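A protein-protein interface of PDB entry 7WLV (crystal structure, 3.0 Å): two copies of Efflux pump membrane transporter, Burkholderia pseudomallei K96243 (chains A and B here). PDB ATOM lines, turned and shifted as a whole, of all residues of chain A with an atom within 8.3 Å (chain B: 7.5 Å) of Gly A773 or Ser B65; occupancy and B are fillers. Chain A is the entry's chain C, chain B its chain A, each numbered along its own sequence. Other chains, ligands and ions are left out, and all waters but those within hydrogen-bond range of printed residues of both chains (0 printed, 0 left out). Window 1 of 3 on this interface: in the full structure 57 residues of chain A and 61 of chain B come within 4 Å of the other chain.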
ATOM      1  N   ASP A 166     -34.471  -2.670 -26.856  1.00  0.00           N
ATOM      2  CA  ASP A 166     -33.794  -3.388 -25.779  1.00  0.00           C
ATOM      3  C   ASP A 166     -34.712  -4.423 -25.131  1.00  0.00           C
ATOM      4  O   ASP A 166     -34.267  -5.519 -24.755  1.00  0.00           O
ATOM      5  CB  ASP A 166     -33.314  -2.388 -24.725  1.00  0.00           C
ATOM      6  CG  ASP A 166     -32.270  -1.412 -25.264  1.00  0.00           C
ATOM      7  OD1 ASP A 166     -32.223  -1.216 -26.496  1.00  0.00           O
ATOM      8  OD2 ASP A 166     -31.518  -0.812 -24.459  1.00  0.00           O
ATOM      9  N   ARG A 242     -20.944  19.660 -21.548  1.00  0.00           N
ATOM     10  CA  ARG A 242     -21.465  19.288 -22.859  1.00  0.00           C
ATOM     11  C   ARG A 242     -22.706  20.113 -23.188  1.00  0.00           C
ATOM     12  O   ARG A 242     -23.456  20.517 -22.294  1.00  0.00           O
ATOM     13  CB  ARG A 242     -21.834  17.804 -22.911  1.00  0.00           C
ATOM     14  CG  ARG A 242     -20.669  16.832 -22.905  1.00  0.00           C
ATOM     15  CD  ARG A 242     -21.001  15.511 -23.613  1.00  0.00           C
ATOM     16  NE  ARG A 242     -19.955  14.518 -23.399  1.00  0.00           N
ATOM     17  CZ  ARG A 242     -20.051  13.239 -23.731  1.00  0.00           C
ATOM     18  NH1 ARG A 242     -21.113  12.769 -24.357  1.00  0.00           N
ATOM     19  NH2 ARG A 242     -19.079  12.404 -23.382  1.00  0.00           N
ATOM     20  N   GLN A 244     -26.482  20.583 -25.059  1.00  0.00           N
ATOM     21  CA  GLN A 244     -27.702  19.788 -25.056  1.00  0.00           C
ATOM     22  C   GLN A 244     -28.628  20.014 -26.245  1.00  0.00           C
ATOM     23  O   GLN A 244     -29.353  19.091 -26.615  1.00  0.00           O
ATOM     24  CB  GLN A 244     -28.484  20.064 -23.764  1.00  0.00           C
ATOM     25  CG  GLN A 244     -27.853  19.414 -22.535  1.00  0.00           C
ATOM     26  CD  GLN A 244     -28.557  19.782 -21.236  1.00  0.00           C
ATOM     27  OE1 GLN A 244     -29.278  20.788 -21.158  1.00  0.00           O
ATOM     28  NE2 GLN A 244     -28.357  18.959 -20.208  1.00  0.00           N
ATOM     29  N   PHE A 769     -22.318  14.361 -27.746  1.00  0.00           N
ATOM     30  CA  PHE A 769     -23.148  15.166 -26.867  1.00  0.00           C
ATOM     31  C   PHE A 769     -24.268  14.319 -26.286  1.00  0.00           C
ATOM     32  O   PHE A 769     -24.686  13.326 -26.876  1.00  0.00           O
ATOM     33  CB  PHE A 769     -23.725  16.380 -27.584  1.00  0.00           C
ATOM     34  CG  PHE A 769     -24.997  16.104 -28.333  1.00  0.00           C
ATOM     35  CD1 PHE A 769     -24.970  15.425 -29.538  1.00  0.00           C
ATOM     36  CD2 PHE A 769     -26.218  16.539 -27.839  1.00  0.00           C
ATOM     37  CE1 PHE A 769     -26.134  15.199 -30.243  1.00  0.00           C
ATOM     38  CE2 PHE A 769     -27.389  16.307 -28.534  1.00  0.00           C
ATOM     39  CZ  PHE A 769     -27.350  15.642 -29.740  1.00  0.00           C
ATOM     40  N   ASN A 770     -24.744  14.728 -25.118  1.00  0.00           N
ATOM     41  CA  ASN A 770     -25.710  13.960 -24.351  1.00  0.00           C
ATOM     42  C   ASN A 770     -27.138  14.435 -24.560  1.00  0.00           C
ATOM     43  O   ASN A 770     -27.416  15.634 -24.651  1.00  0.00           O
ATOM     44  CB  ASN A 770     -25.364  13.976 -22.868  1.00  0.00           C
ATOM     45  CG  ASN A 770     -24.245  13.007 -22.541  1.00  0.00           C
ATOM     46  OD1 ASN A 770     -23.067  13.357 -22.611  1.00  0.00           O
ATOM     47  ND2 ASN A 770     -24.608  11.764 -22.219  1.00  0.00           N
ATOM     48  N   ARG A 771     -28.028  13.458 -24.657  1.00  0.00           N
ATOM     49  CA  ARG A 771     -29.448  13.658 -24.894  1.00  0.00           C
ATOM     50  C   ARG A 771     -30.176  12.494 -24.245  1.00  0.00           C
ATOM     51  O   ARG A 771     -29.940  11.342 -24.623  1.00  0.00           O
ATOM     52  CB  ARG A 771     -29.736  13.712 -26.385  1.00  0.00           C
ATOM     53  CG  ARG A 771     -31.172  13.914 -26.746  1.00  0.00           C
ATOM     54  CD  ARG A 771     -31.287  14.000 -28.237  1.00  0.00           C
ATOM     55  NE  ARG A 771     -32.567  14.565 -28.635  1.00  0.00           N
ATOM     56  CZ  ARG A 771     -33.676  13.867 -28.807  1.00  0.00           C
ATOM     57  NH1 ARG A 771     -33.708  12.560 -28.590  1.00  0.00           N
ATOM     58  NH2 ARG A 771     -34.783  14.497 -29.193  1.00  0.00           N
ATOM     59  N   PHE A 772     -31.035  12.789 -23.267  1.00  0.00           N
ATOM     60  CA  PHE A 772     -31.718  11.764 -22.467  1.00  0.00           C
ATOM     61  C   PHE A 772     -30.728  10.799 -21.808  1.00  0.00           C
ATOM     62  O   PHE A 772     -30.962   9.590 -21.743  1.00  0.00           O
ATOM     63  CB  PHE A 772     -32.721  10.978 -23.317  1.00  0.00           C
ATOM     64  CG  PHE A 772     -33.782  11.824 -23.969  1.00  0.00           C
ATOM     65  CD1 PHE A 772     -33.949  13.165 -23.630  1.00  0.00           C
ATOM     66  CD2 PHE A 772     -34.638  11.262 -24.909  1.00  0.00           C
ATOM     67  CE1 PHE A 772     -34.930  13.933 -24.235  1.00  0.00           C
ATOM     68  CE2 PHE A 772     -35.628  12.019 -25.510  1.00  0.00           C
ATOM     69  CZ  PHE A 772     -35.774  13.356 -25.174  1.00  0.00           C
ATOM     70  N   GLY A 773     -29.617  11.337 -21.300  1.00  0.00           N
ATOM     71  CA  GLY A 773     -28.587  10.504 -20.698  1.00  0.00           C
ATOM     72  C   GLY A 773     -27.822   9.611 -21.656  1.00  0.00           C
ATOM     73  O   GLY A 773     -27.019   8.786 -21.210  1.00  0.00           O
ATOM     74  N   ARG A 774     -28.048   9.764 -22.962  1.00  0.00           N
ATOM     75  CA  ARG A 774     -27.445   8.949 -24.005  1.00  0.00           C
ATOM     76  C   ARG A 774     -26.449   9.747 -24.831  1.00  0.00           C
ATOM     77  O   ARG A 774     -26.572  10.967 -24.982  1.00  0.00           O
ATOM     78  CB  ARG A 774     -28.511   8.391 -24.936  1.00  0.00           C
ATOM     79  CG  ARG A 774     -29.374   7.321 -24.355  1.00  0.00           C
ATOM     80  CD  ARG A 774     -30.382   7.022 -25.393  1.00  0.00           C
ATOM     81  NE  ARG A 774     -29.717   6.850 -26.680  1.00  0.00           N
ATOM     82  CZ  ARG A 774     -29.312   5.702 -27.203  1.00  0.00           C
ATOM     83  NH1 ARG A 774     -29.494   4.547 -26.577  1.00  0.00           N
ATOM     84  NH2 ARG A 774     -28.688   5.715 -28.380  1.00  0.00           N
ATOM     85  N   VAL A 775     -25.485   9.049 -25.385  1.00  0.00           N
ATOM     86  CA  VAL A 775     -24.452   9.684 -26.189  1.00  0.00           C
ATOM     87  C   VAL A 775     -24.903   9.722 -27.643  1.00  0.00           C
ATOM     88  O   VAL A 775     -25.520   8.777 -28.143  1.00  0.00           O
ATOM     89  CB  VAL A 775     -23.111   8.951 -26.020  1.00  0.00           C
ATOM     90  CG1 VAL A 775     -22.548   9.229 -24.633  1.00  0.00           C
ATOM     91  CG2 VAL A 775     -23.295   7.462 -26.227  1.00  0.00           C
ATOM     92  N   TYR A 776     -24.652  10.848 -28.303  1.00  0.00           N
ATOM     93  CA  TYR A 776     -24.965  11.027 -29.709  1.00  0.00           C
ATOM     94  C   TYR A 776     -23.808  11.764 -30.379  1.00  0.00           C
ATOM     95  O   TYR A 776     -23.025  12.454 -29.729  1.00  0.00           O
ATOM     96  CB  TYR A 776     -26.282  11.782 -29.888  1.00  0.00           C
ATOM     97  CG  TYR A 776     -27.497  10.949 -29.571  1.00  0.00           C
ATOM     98  CD1 TYR A 776     -27.908   9.933 -30.420  1.00  0.00           C
ATOM     99  CD2 TYR A 776     -28.234  11.174 -28.424  1.00  0.00           C
ATOM    100  CE1 TYR A 776     -29.024   9.163 -30.138  1.00  0.00           C
ATOM    101  CE2 TYR A 776     -29.356  10.412 -28.132  1.00  0.00           C
ATOM    102  CZ  TYR A 776     -29.745   9.411 -28.995  1.00  0.00           C
ATOM    103  OH  TYR A 776     -30.859   8.656 -28.719  1.00  0.00           O
ATOM    104  N   LYS B  57     -23.059  11.758 -11.576  1.00  0.00           N
ATOM    105  CA  LYS B  57     -23.965  11.934 -12.708  1.00  0.00           C
ATOM    106  C   LYS B  57     -23.215  11.841 -14.038  1.00  0.00           C
ATOM    107  O   LYS B  57     -23.644  11.123 -14.964  1.00  0.00           O
ATOM    108  CB  LYS B  57     -24.691  13.279 -12.563  1.00  0.00           C
ATOM    109  CG  LYS B  57     -25.599  13.303 -11.339  1.00  0.00           C
ATOM    110  CD  LYS B  57     -26.328  14.611 -11.137  1.00  0.00           C
ATOM    111  CE  LYS B  57     -25.472  15.640 -10.413  1.00  0.00           C
ATOM    112  NZ  LYS B  57     -26.235  16.863 -10.028  1.00  0.00           N
ATOM    113  N   VAL B  58     -22.048  12.492 -14.114  1.00  0.00           N
ATOM    114  CA  VAL B  58     -21.229  12.428 -15.321  1.00  0.00           C
ATOM    115  C   VAL B  58     -20.784  10.998 -15.584  1.00  0.00           C
ATOM    116  O   VAL B  58     -20.768  10.544 -16.734  1.00  0.00           O
ATOM    117  CB  VAL B  58     -20.019  13.371 -15.209  1.00  0.00           C
ATOM    118  CG1 VAL B  58     -19.183  13.305 -16.483  1.00  0.00           C
ATOM    119  CG2 VAL B  58     -20.477  14.784 -14.916  1.00  0.00           C
ATOM    120  N   ILE B  59     -20.407  10.269 -14.526  1.00  0.00           N
ATOM    121  CA  ILE B  59     -19.971   8.885 -14.692  1.00  0.00           C
ATOM    122  C   ILE B  59     -21.123   8.021 -15.186  1.00  0.00           C
ATOM    123  O   ILE B  59     -20.936   7.124 -16.016  1.00  0.00           O
ATOM    124  CB  ILE B  59     -19.376   8.344 -13.387  1.00  0.00           C
ATOM    125  CG1 ILE B  59     -18.280   9.274 -12.902  1.00  0.00           C
ATOM    126  CG2 ILE B  59     -18.695   7.045 -13.668  1.00  0.00           C
ATOM    127  CD1 ILE B  59     -17.629   8.833 -11.638  1.00  0.00           C
ATOM    128  N   ALA B  60     -22.323   8.243 -14.647  1.00  0.00           N
ATOM    129  CA  ALA B  60     -23.482   7.472 -15.088  1.00  0.00           C
ATOM    130  C   ALA B  60     -23.791   7.716 -16.561  1.00  0.00           C
ATOM    131  O   ALA B  60     -24.147   6.777 -17.287  1.00  0.00           O
ATOM    132  CB  ALA B  60     -24.696   7.804 -14.224  1.00  0.00           C
ATOM    133  N   GLU B  61     -23.632   8.962 -17.032  1.00  0.00           N
ATOM    134  CA  GLU B  61     -24.112   9.314 -18.369  1.00  0.00           C
ATOM    135  C   GLU B  61     -23.067   9.270 -19.478  1.00  0.00           C
ATOM    136  O   GLU B  61     -23.434   8.985 -20.619  1.00  0.00           O
ATOM    137  CB  GLU B  61     -24.731  10.708 -18.377  1.00  0.00           C
ATOM    138  CG  GLU B  61     -25.913  10.849 -17.483  1.00  0.00           C
ATOM    139  CD  GLU B  61     -26.407  12.273 -17.442  1.00  0.00           C
ATOM    140  OE1 GLU B  61     -26.023  13.040 -18.362  1.00  0.00           O
ATOM    141  OE2 GLU B  61     -27.189  12.614 -16.517  1.00  0.00           O
ATOM    142  N   THR B  62     -21.788   9.529 -19.215  1.00  0.00           N
ATOM    143  CA  THR B  62     -20.807   9.515 -20.294  1.00  0.00           C
ATOM    144  C   THR B  62     -19.940   8.268 -20.299  1.00  0.00           C
ATOM    145  O   THR B  62     -19.247   8.016 -21.294  1.00  0.00           O
ATOM    146  CB  THR B  62     -19.894  10.747 -20.225  1.00  0.00           C
ATOM    147  OG1 THR B  62     -18.952  10.590 -19.155  1.00  0.00           O
ATOM    148  CG2 THR B  62     -20.708  12.007 -20.002  1.00  0.00           C
ATOM    149  N   VAL B  63     -19.970   7.488 -19.223  1.00  0.00           N
ATOM    150  CA  VAL B  63     -19.183   6.265 -19.099  1.00  0.00           C
ATOM    151  C   VAL B  63     -20.084   5.039 -19.055  1.00  0.00           C
ATOM    152  O   VAL B  63     -19.983   4.147 -19.900  1.00  0.00           O
ATOM    153  CB  VAL B  63     -18.278   6.325 -17.847  1.00  0.00           C
ATOM    154  CG1 VAL B  63     -17.411   5.058 -17.728  1.00  0.00           C
ATOM    155  CG2 VAL B  63     -17.470   7.633 -17.795  1.00  0.00           C
ATOM    156  N   ALA B  64     -20.956   4.965 -18.050  1.00  0.00           N
ATOM    157  CA  ALA B  64     -21.780   3.785 -17.836  1.00  0.00           C
ATOM    158  C   ALA B  64     -22.763   3.553 -18.975  1.00  0.00           C
ATOM    159  O   ALA B  64     -22.981   2.406 -19.377  1.00  0.00           O
ATOM    160  CB  ALA B  64     -22.509   3.914 -16.503  1.00  0.00           C
ATOM    161  N   SER B  65     -23.408   4.618 -19.472  1.00  0.00           N
ATOM    162  CA  SER B  65     -24.500   4.441 -20.433  1.00  0.00           C
ATOM    163  C   SER B  65     -24.063   3.810 -21.751  1.00  0.00           C
ATOM    164  O   SER B  65     -24.744   2.878 -22.209  1.00  0.00           O
ATOM    165  CB  SER B  65     -25.258   5.762 -20.640  1.00  0.00           C
ATOM    166  OG  SER B  65     -24.414   6.896 -20.603  1.00  0.00           O
ATOM    167  N   PRO B  66     -22.997   4.257 -22.426  1.00  0.00           N
ATOM    168  CA  PRO B  66     -22.562   3.515 -23.626  1.00  0.00           C
ATOM    169  C   PRO B  66     -22.204   2.059 -23.344  1.00  0.00           C
ATOM    170  O   PRO B  66     -22.517   1.161 -24.146  1.00  0.00           O
ATOM    171  CB  PRO B  66     -21.348   4.322 -24.112  1.00  0.00           C
ATOM    172  CG  PRO B  66     -20.945   5.173 -22.945  1.00  0.00           C
ATOM    173  CD  PRO B  66     -22.199   5.478 -22.229  1.00  0.00           C
ATOM    174  N   LEU B  67     -21.551   1.803 -22.208  1.00  0.00           N
ATOM    175  CA  LEU B  67     -21.211   0.436 -21.835  1.00  0.00           C
ATOM    176  C   LEU B  67     -22.464  -0.417 -21.677  1.00  0.00           C
ATOM    177  O   LEU B  67     -22.506  -1.566 -22.134  1.00  0.00           O
ATOM    178  CB  LEU B  67     -20.401   0.452 -20.544  1.00  0.00           C
ATOM    179  CG  LEU B  67     -18.989   0.992 -20.708  1.00  0.00           C
ATOM    180  CD1 LEU B  67     -18.369   1.180 -19.344  1.00  0.00           C
ATOM    181  CD2 LEU B  67     -18.151   0.048 -21.553  1.00  0.00           C
ATOM    182  N   GLU B  68     -23.493   0.129 -21.030  1.00  0.00           N
ATOM    183  CA  GLU B  68     -24.744  -0.600 -20.908  1.00  0.00           C
ATOM    184  C   GLU B  68     -25.386  -0.798 -22.269  1.00  0.00           C
ATOM    185  O   GLU B  68     -25.916  -1.876 -22.564  1.00  0.00           O
ATOM    186  CB  GLU B  68     -25.709   0.158 -20.006  1.00  0.00           C
ATOM    187  CG  GLU B  68     -25.223   0.420 -18.613  1.00  0.00           C
ATOM    188  CD  GLU B  68     -25.967   1.584 -17.967  1.00  0.00           C
ATOM    189  OE1 GLU B  68     -26.721   2.293 -18.679  1.00  0.00           O
ATOM    190  OE2 GLU B  68     -25.826   1.778 -16.740  1.00  0.00           O
ATOM    191  N   GLU B  69     -25.302   0.219 -23.129  1.00  0.00           N
ATOM    192  CA  GLU B  69     -25.935   0.132 -24.437  1.00  0.00           C
ATOM    193  C   GLU B  69     -25.327  -0.993 -25.258  1.00  0.00           C
ATOM    194  O   GLU B  69     -26.030  -1.670 -26.016  1.00  0.00           O
ATOM    195  CB  GLU B  69     -25.864   1.489 -25.143  1.00  0.00           C
ATOM    196  CG  GLU B  69     -26.363   1.488 -26.585  1.00  0.00           C
ATOM    197  CD  GLU B  69     -26.641   2.893 -27.126  1.00  0.00           C
ATOM    198  OE1 GLU B  69     -26.390   3.878 -26.397  1.00  0.00           O
ATOM    199  OE2 GLU B  69     -27.118   3.008 -28.282  1.00  0.00           O
ATOM    200  N   GLN B  70     -24.025  -1.209 -25.122  1.00  0.00           N
ATOM    201  CA  GLN B  70     -23.414  -2.352 -25.800  1.00  0.00           C
ATOM    202  C   GLN B  70     -23.701  -3.679 -25.095  1.00  0.00           C
ATOM    203  O   GLN B  70     -23.903  -4.701 -25.760  1.00  0.00           O
ATOM    204  CB  GLN B  70     -21.918  -2.128 -25.947  1.00  0.00           C
ATOM    205  CG  GLN B  70     -21.671  -1.038 -26.937  1.00  0.00           C
ATOM    206  CD  GLN B  70     -22.020  -1.490 -28.329  1.00  0.00           C
ATOM    207  OE1 GLN B  70     -21.779  -2.637 -28.693  1.00  0.00           O
ATOM    208  NE2 GLN B  70     -22.639  -0.607 -29.104  1.00  0.00           N
ATOM    209  N   ILE B  71     -23.675  -3.692 -23.757  1.00  0.00           N
ATOM    210  CA  ILE B  71     -23.870  -4.929 -23.001  1.00  0.00           C
ATOM    211  C   ILE B  71     -25.304  -5.444 -23.103  1.00  0.00           C
ATOM    212  O   ILE B  71     -25.526  -6.655 -23.190  1.00  0.00           O
ATOM    213  CB  ILE B  71     -23.434  -4.720 -21.538  1.00  0.00           C
ATOM    214  CG1 ILE B  71     -21.911  -4.647 -21.458  1.00  0.00           C
ATOM    215  CG2 ILE B  71     -23.964  -5.808 -20.640  1.00  0.00           C
ATOM    216  CD1 ILE B  71     -21.386  -4.231 -20.121  1.00  0.00           C
ATOM    217  N   MET B  80     -29.049  -6.272 -15.531  1.00  0.00           N
ATOM    218  CA  MET B  80     -27.764  -5.606 -15.351  1.00  0.00           C
ATOM    219  C   MET B  80     -27.944  -4.325 -14.553  1.00  0.00           C
ATOM    220  O   MET B  80     -29.012  -3.707 -14.581  1.00  0.00           O
ATOM    221  CB  MET B  80     -27.100  -5.296 -16.696  1.00  0.00           C
ATOM    222  CG  MET B  80     -27.947  -4.421 -17.586  1.00  0.00           C
ATOM    223  SD  MET B  80     -27.052  -3.818 -19.029  1.00  0.00           S
ATOM    224  CE  MET B  80     -25.500  -3.383 -18.251  1.00  0.00           C
ATOM    225  N   SER B  82     -25.395  -0.750 -13.412  1.00  0.00           N
ATOM    226  CA  SER B  82     -24.165   0.015 -13.272  1.00  0.00           C
ATOM    227  C   SER B  82     -24.268   0.933 -12.057  1.00  0.00           C
ATOM    228  O   SER B  82     -25.357   1.381 -11.690  1.00  0.00           O
ATOM    229  CB  SER B  82     -23.905   0.825 -14.533  1.00  0.00           C
ATOM    230  OG  SER B  82     -24.937   1.775 -14.716  1.00  0.00           O
ATOM    231  N   MET B  90     -16.648   3.400 -11.455  1.00  0.00           N
ATOM    232  CA  MET B  90     -17.840   2.933 -12.143  1.00  0.00           C
ATOM    233  C   MET B  90     -17.788   1.416 -12.196  1.00  0.00           C
ATOM    234  O   MET B  90     -16.789   0.855 -12.662  1.00  0.00           O
ATOM    235  CB  MET B  90     -17.912   3.509 -13.553  1.00  0.00           C
ATOM    236  CG  MET B  90     -19.266   3.352 -14.229  1.00  0.00           C
ATOM    237  SD  MET B  90     -19.534   1.695 -14.927  1.00  0.00           S
ATOM    238  CE  MET B  90     -17.992   1.430 -15.818  1.00  0.00           C
ATOM    239  N   ILE B  92     -20.122  -2.035 -13.340  1.00  0.00           N
ATOM    240  CA  ILE B  92     -21.268  -2.664 -13.989  1.00  0.00           C
ATOM    241  C   ILE B  92     -21.308  -4.142 -13.619  1.00  0.00           C
ATOM    242  O   ILE B  92     -20.295  -4.841 -13.730  1.00  0.00           O
ATOM    243  CB  ILE B  92     -21.217  -2.491 -15.513  1.00  0.00           C
ATOM    244  CG1 ILE B  92     -21.339  -1.011 -15.873  1.00  0.00           C
ATOM    245  CG2 ILE B  92     -22.345  -3.264 -16.147  1.00  0.00           C
ATOM    246  CD1 ILE B  92     -21.337  -0.710 -17.358  1.00  0.00           C
ATOM    247  N   ALA B 116     -17.866  -1.039 -26.989  1.00  0.00           N
ATOM    248  CA  ALA B 116     -18.212   0.268 -26.434  1.00  0.00           C
ATOM    249  C   ALA B 116     -17.006   1.169 -26.207  1.00  0.00           C
ATOM    250  O   ALA B 116     -17.162   2.394 -26.200  1.00  0.00           O
ATOM    251  CB  ALA B 116     -18.947   0.101 -25.108  1.00  0.00           C
ATOM    252  N   LEU B 120     -16.045   5.974 -24.783  1.00  0.00           N
ATOM    253  CA  LEU B 120     -15.700   6.428 -23.444  1.00  0.00           C
ATOM    254  C   LEU B 120     -14.814   7.670 -23.501  1.00  0.00           C
ATOM    255  O   LEU B 120     -14.105   7.888 -24.484  1.00  0.00           O
ATOM    256  CB  LEU B 120     -14.968   5.321 -22.673  1.00  0.00           C
ATOM    257  CG  LEU B 120     -15.673   4.067 -22.122  1.00  0.00           C
ATOM    258  CD1 LEU B 120     -16.622   4.483 -21.041  1.00  0.00           C
ATOM    259  CD2 LEU B 120     -16.427   3.255 -23.147  1.00  0.00           C
ATOM    260  N   ALA B 697     -37.027  10.050 -19.338  1.00  0.00           N
ATOM    261  CA  ALA B 697     -36.253  11.274 -19.126  1.00  0.00           C
ATOM    262  C   ALA B 697     -36.848  12.127 -18.007  1.00  0.00           C
ATOM    263  O   ALA B 697     -36.807  13.359 -18.036  1.00  0.00           O
ATOM    264  CB  ALA B 697     -36.134  12.082 -20.420  1.00  0.00           C
ATOM    265  N   TYR B 700     -33.840  13.371 -12.074  1.00  0.00           N
ATOM    266  CA  TYR B 700     -33.479  12.713 -10.815  1.00  0.00           C
ATOM    267  C   TYR B 700     -34.384  13.193  -9.691  1.00  0.00           C
ATOM    268  O   TYR B 700     -34.765  12.415  -8.808  1.00  0.00           O
ATOM    269  CB  TYR B 700     -32.038  13.000 -10.389  1.00  0.00           C
ATOM    270  CG  TYR B 700     -30.897  12.449 -11.196  1.00  0.00           C
ATOM    271  CD1 TYR B 700     -30.435  11.151 -10.998  1.00  0.00           C
ATOM    272  CD2 TYR B 700     -30.216  13.264 -12.094  1.00  0.00           C
ATOM    273  CE1 TYR B 700     -29.354  10.669 -11.723  1.00  0.00           C
ATOM    274  CE2 TYR B 700     -29.148  12.793 -12.820  1.00  0.00           C
ATOM    275  CZ  TYR B 700     -28.717  11.504 -12.634  1.00  0.00           C
ATOM    276  OH  TYR B 700     -27.642  11.083 -13.372  1.00  0.00           O
ATOM    277  N   ARG B 825     -27.892   2.742 -12.273  1.00  0.00           N
ATOM    278  CA  ARG B 825     -28.708   2.508 -13.463  1.00  0.00           C
ATOM    279  C   ARG B 825     -28.980   1.014 -13.595  1.00  0.00           C
ATOM    280  O   ARG B 825     -28.055   0.235 -13.842  1.00  0.00           O
ATOM    281  CB  ARG B 825     -28.010   3.037 -14.715  1.00  0.00           C
ATOM    282  CG  ARG B 825     -27.904   4.525 -14.823  1.00  0.00           C
ATOM    283  CD  ARG B 825     -26.898   4.893 -15.891  1.00  0.00           C
ATOM    284  NE  ARG B 825     -27.365   4.567 -17.231  1.00  0.00           N
ATOM    285  CZ  ARG B 825     -28.005   5.400 -18.042  1.00  0.00           C
ATOM    286  NH1 ARG B 825     -28.318   6.637 -17.667  1.00  0.00           N
ATOM    287  NH2 ARG B 825     -28.318   4.991 -19.269  1.00  0.00           N
ATOM    288  N   ALA B 828     -30.188  -0.257 -17.851  1.00  0.00           N
ATOM    289  CA  ALA B 828     -29.980   0.945 -18.657  1.00  0.00           C
ATOM    290  C   ALA B 828     -30.993   2.037 -18.347  1.00  0.00           C
ATOM    291  O   ALA B 828     -31.192   2.950 -19.155  1.00  0.00           O
ATOM    292  CB  ALA B 828     -29.992   0.643 -20.159  1.00  0.00           C
ATOM    293  N   THR B 830     -32.008   4.819 -15.250  1.00  0.00           N
ATOM    294  CA  THR B 830     -31.760   5.403 -13.940  1.00  0.00           C
ATOM    295  C   THR B 830     -32.804   4.871 -12.963  1.00  0.00           C
ATOM    296  O   THR B 830     -33.999   4.850 -13.276  1.00  0.00           O
ATOM    297  CB  THR B 830     -31.842   6.924 -14.034  1.00  0.00           C
ATOM    298  OG1 THR B 830     -30.785   7.409 -14.859  1.00  0.00           O
ATOM    299  CG2 THR B 830     -31.702   7.547 -12.671  1.00  0.00           C
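NH1 of Arg A242 lies within hydrogen-bond range of OD1 of Asn A770 (2.7 Å). O of Val B58 lies within hydrogen-bond range of OG1 of Thr B62, 3.0 Å away. The backbone NH of Ser B65 is in hydrogen-bond range of the backbone carbonyl oxygen of Ala B60 (3.2 Å). ND2 of Asn A770 lies close to O of Arg A774 (3.5 Å). The guanidinium group (NE) of Arg A774 is in hydrogen-bond range of the side-chain hydroxyl (OH) of Tyr A776.
No position is printed for both chains.
Arg A242 touches Thr B62. OD1 of Asn A770 touches CG2 of Thr B62, at 3.8 Å. Gly A773 touches Glu B61 (O to O, 3.6 Å).
Printed residues of chain A that touch a printed residue of chain B: Arg A242, Asn A770, Gly A773 and Arg A774. Among the printed residues, 6 pairs touch across the chains. Among the printed residues, Asp or Glu carboxylates within 4 Å of a Lys or Arg side-chain nitrogen of the other chain: Arg A774 with Glu B69.
Gly A773 touches just these residues of chain B: Glu B61 (3.6 Å) and Ser B65 (3.3 Å). Printed residues of chain B within 4 Å of Arg A774: Glu B69 (3.1 Å). Lys B57 touches none of the printed residues of chain A. Of chain A, only Gly A773 comes within 4 Å of Ser B65. Of the printed residues of chain A, Glu B69 touches Arg A774 (3.1 Å). The nearest residue of chain B that does not touch Gly A773 is Arg B825 (4.3 Å).
OE2 of Glu B69 lies within salt-bridge range of NH2 of Arg A774. O of Glu B61 sits at hydrogen-bond distance from ND2 of Asn A770 (3.4 Å). The backbone carbonyl oxygen (O) of Gly A773 is in hydrogen-bond range of the side-chain hydroxyl (OG) of Ser B65 (3.3 Å).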
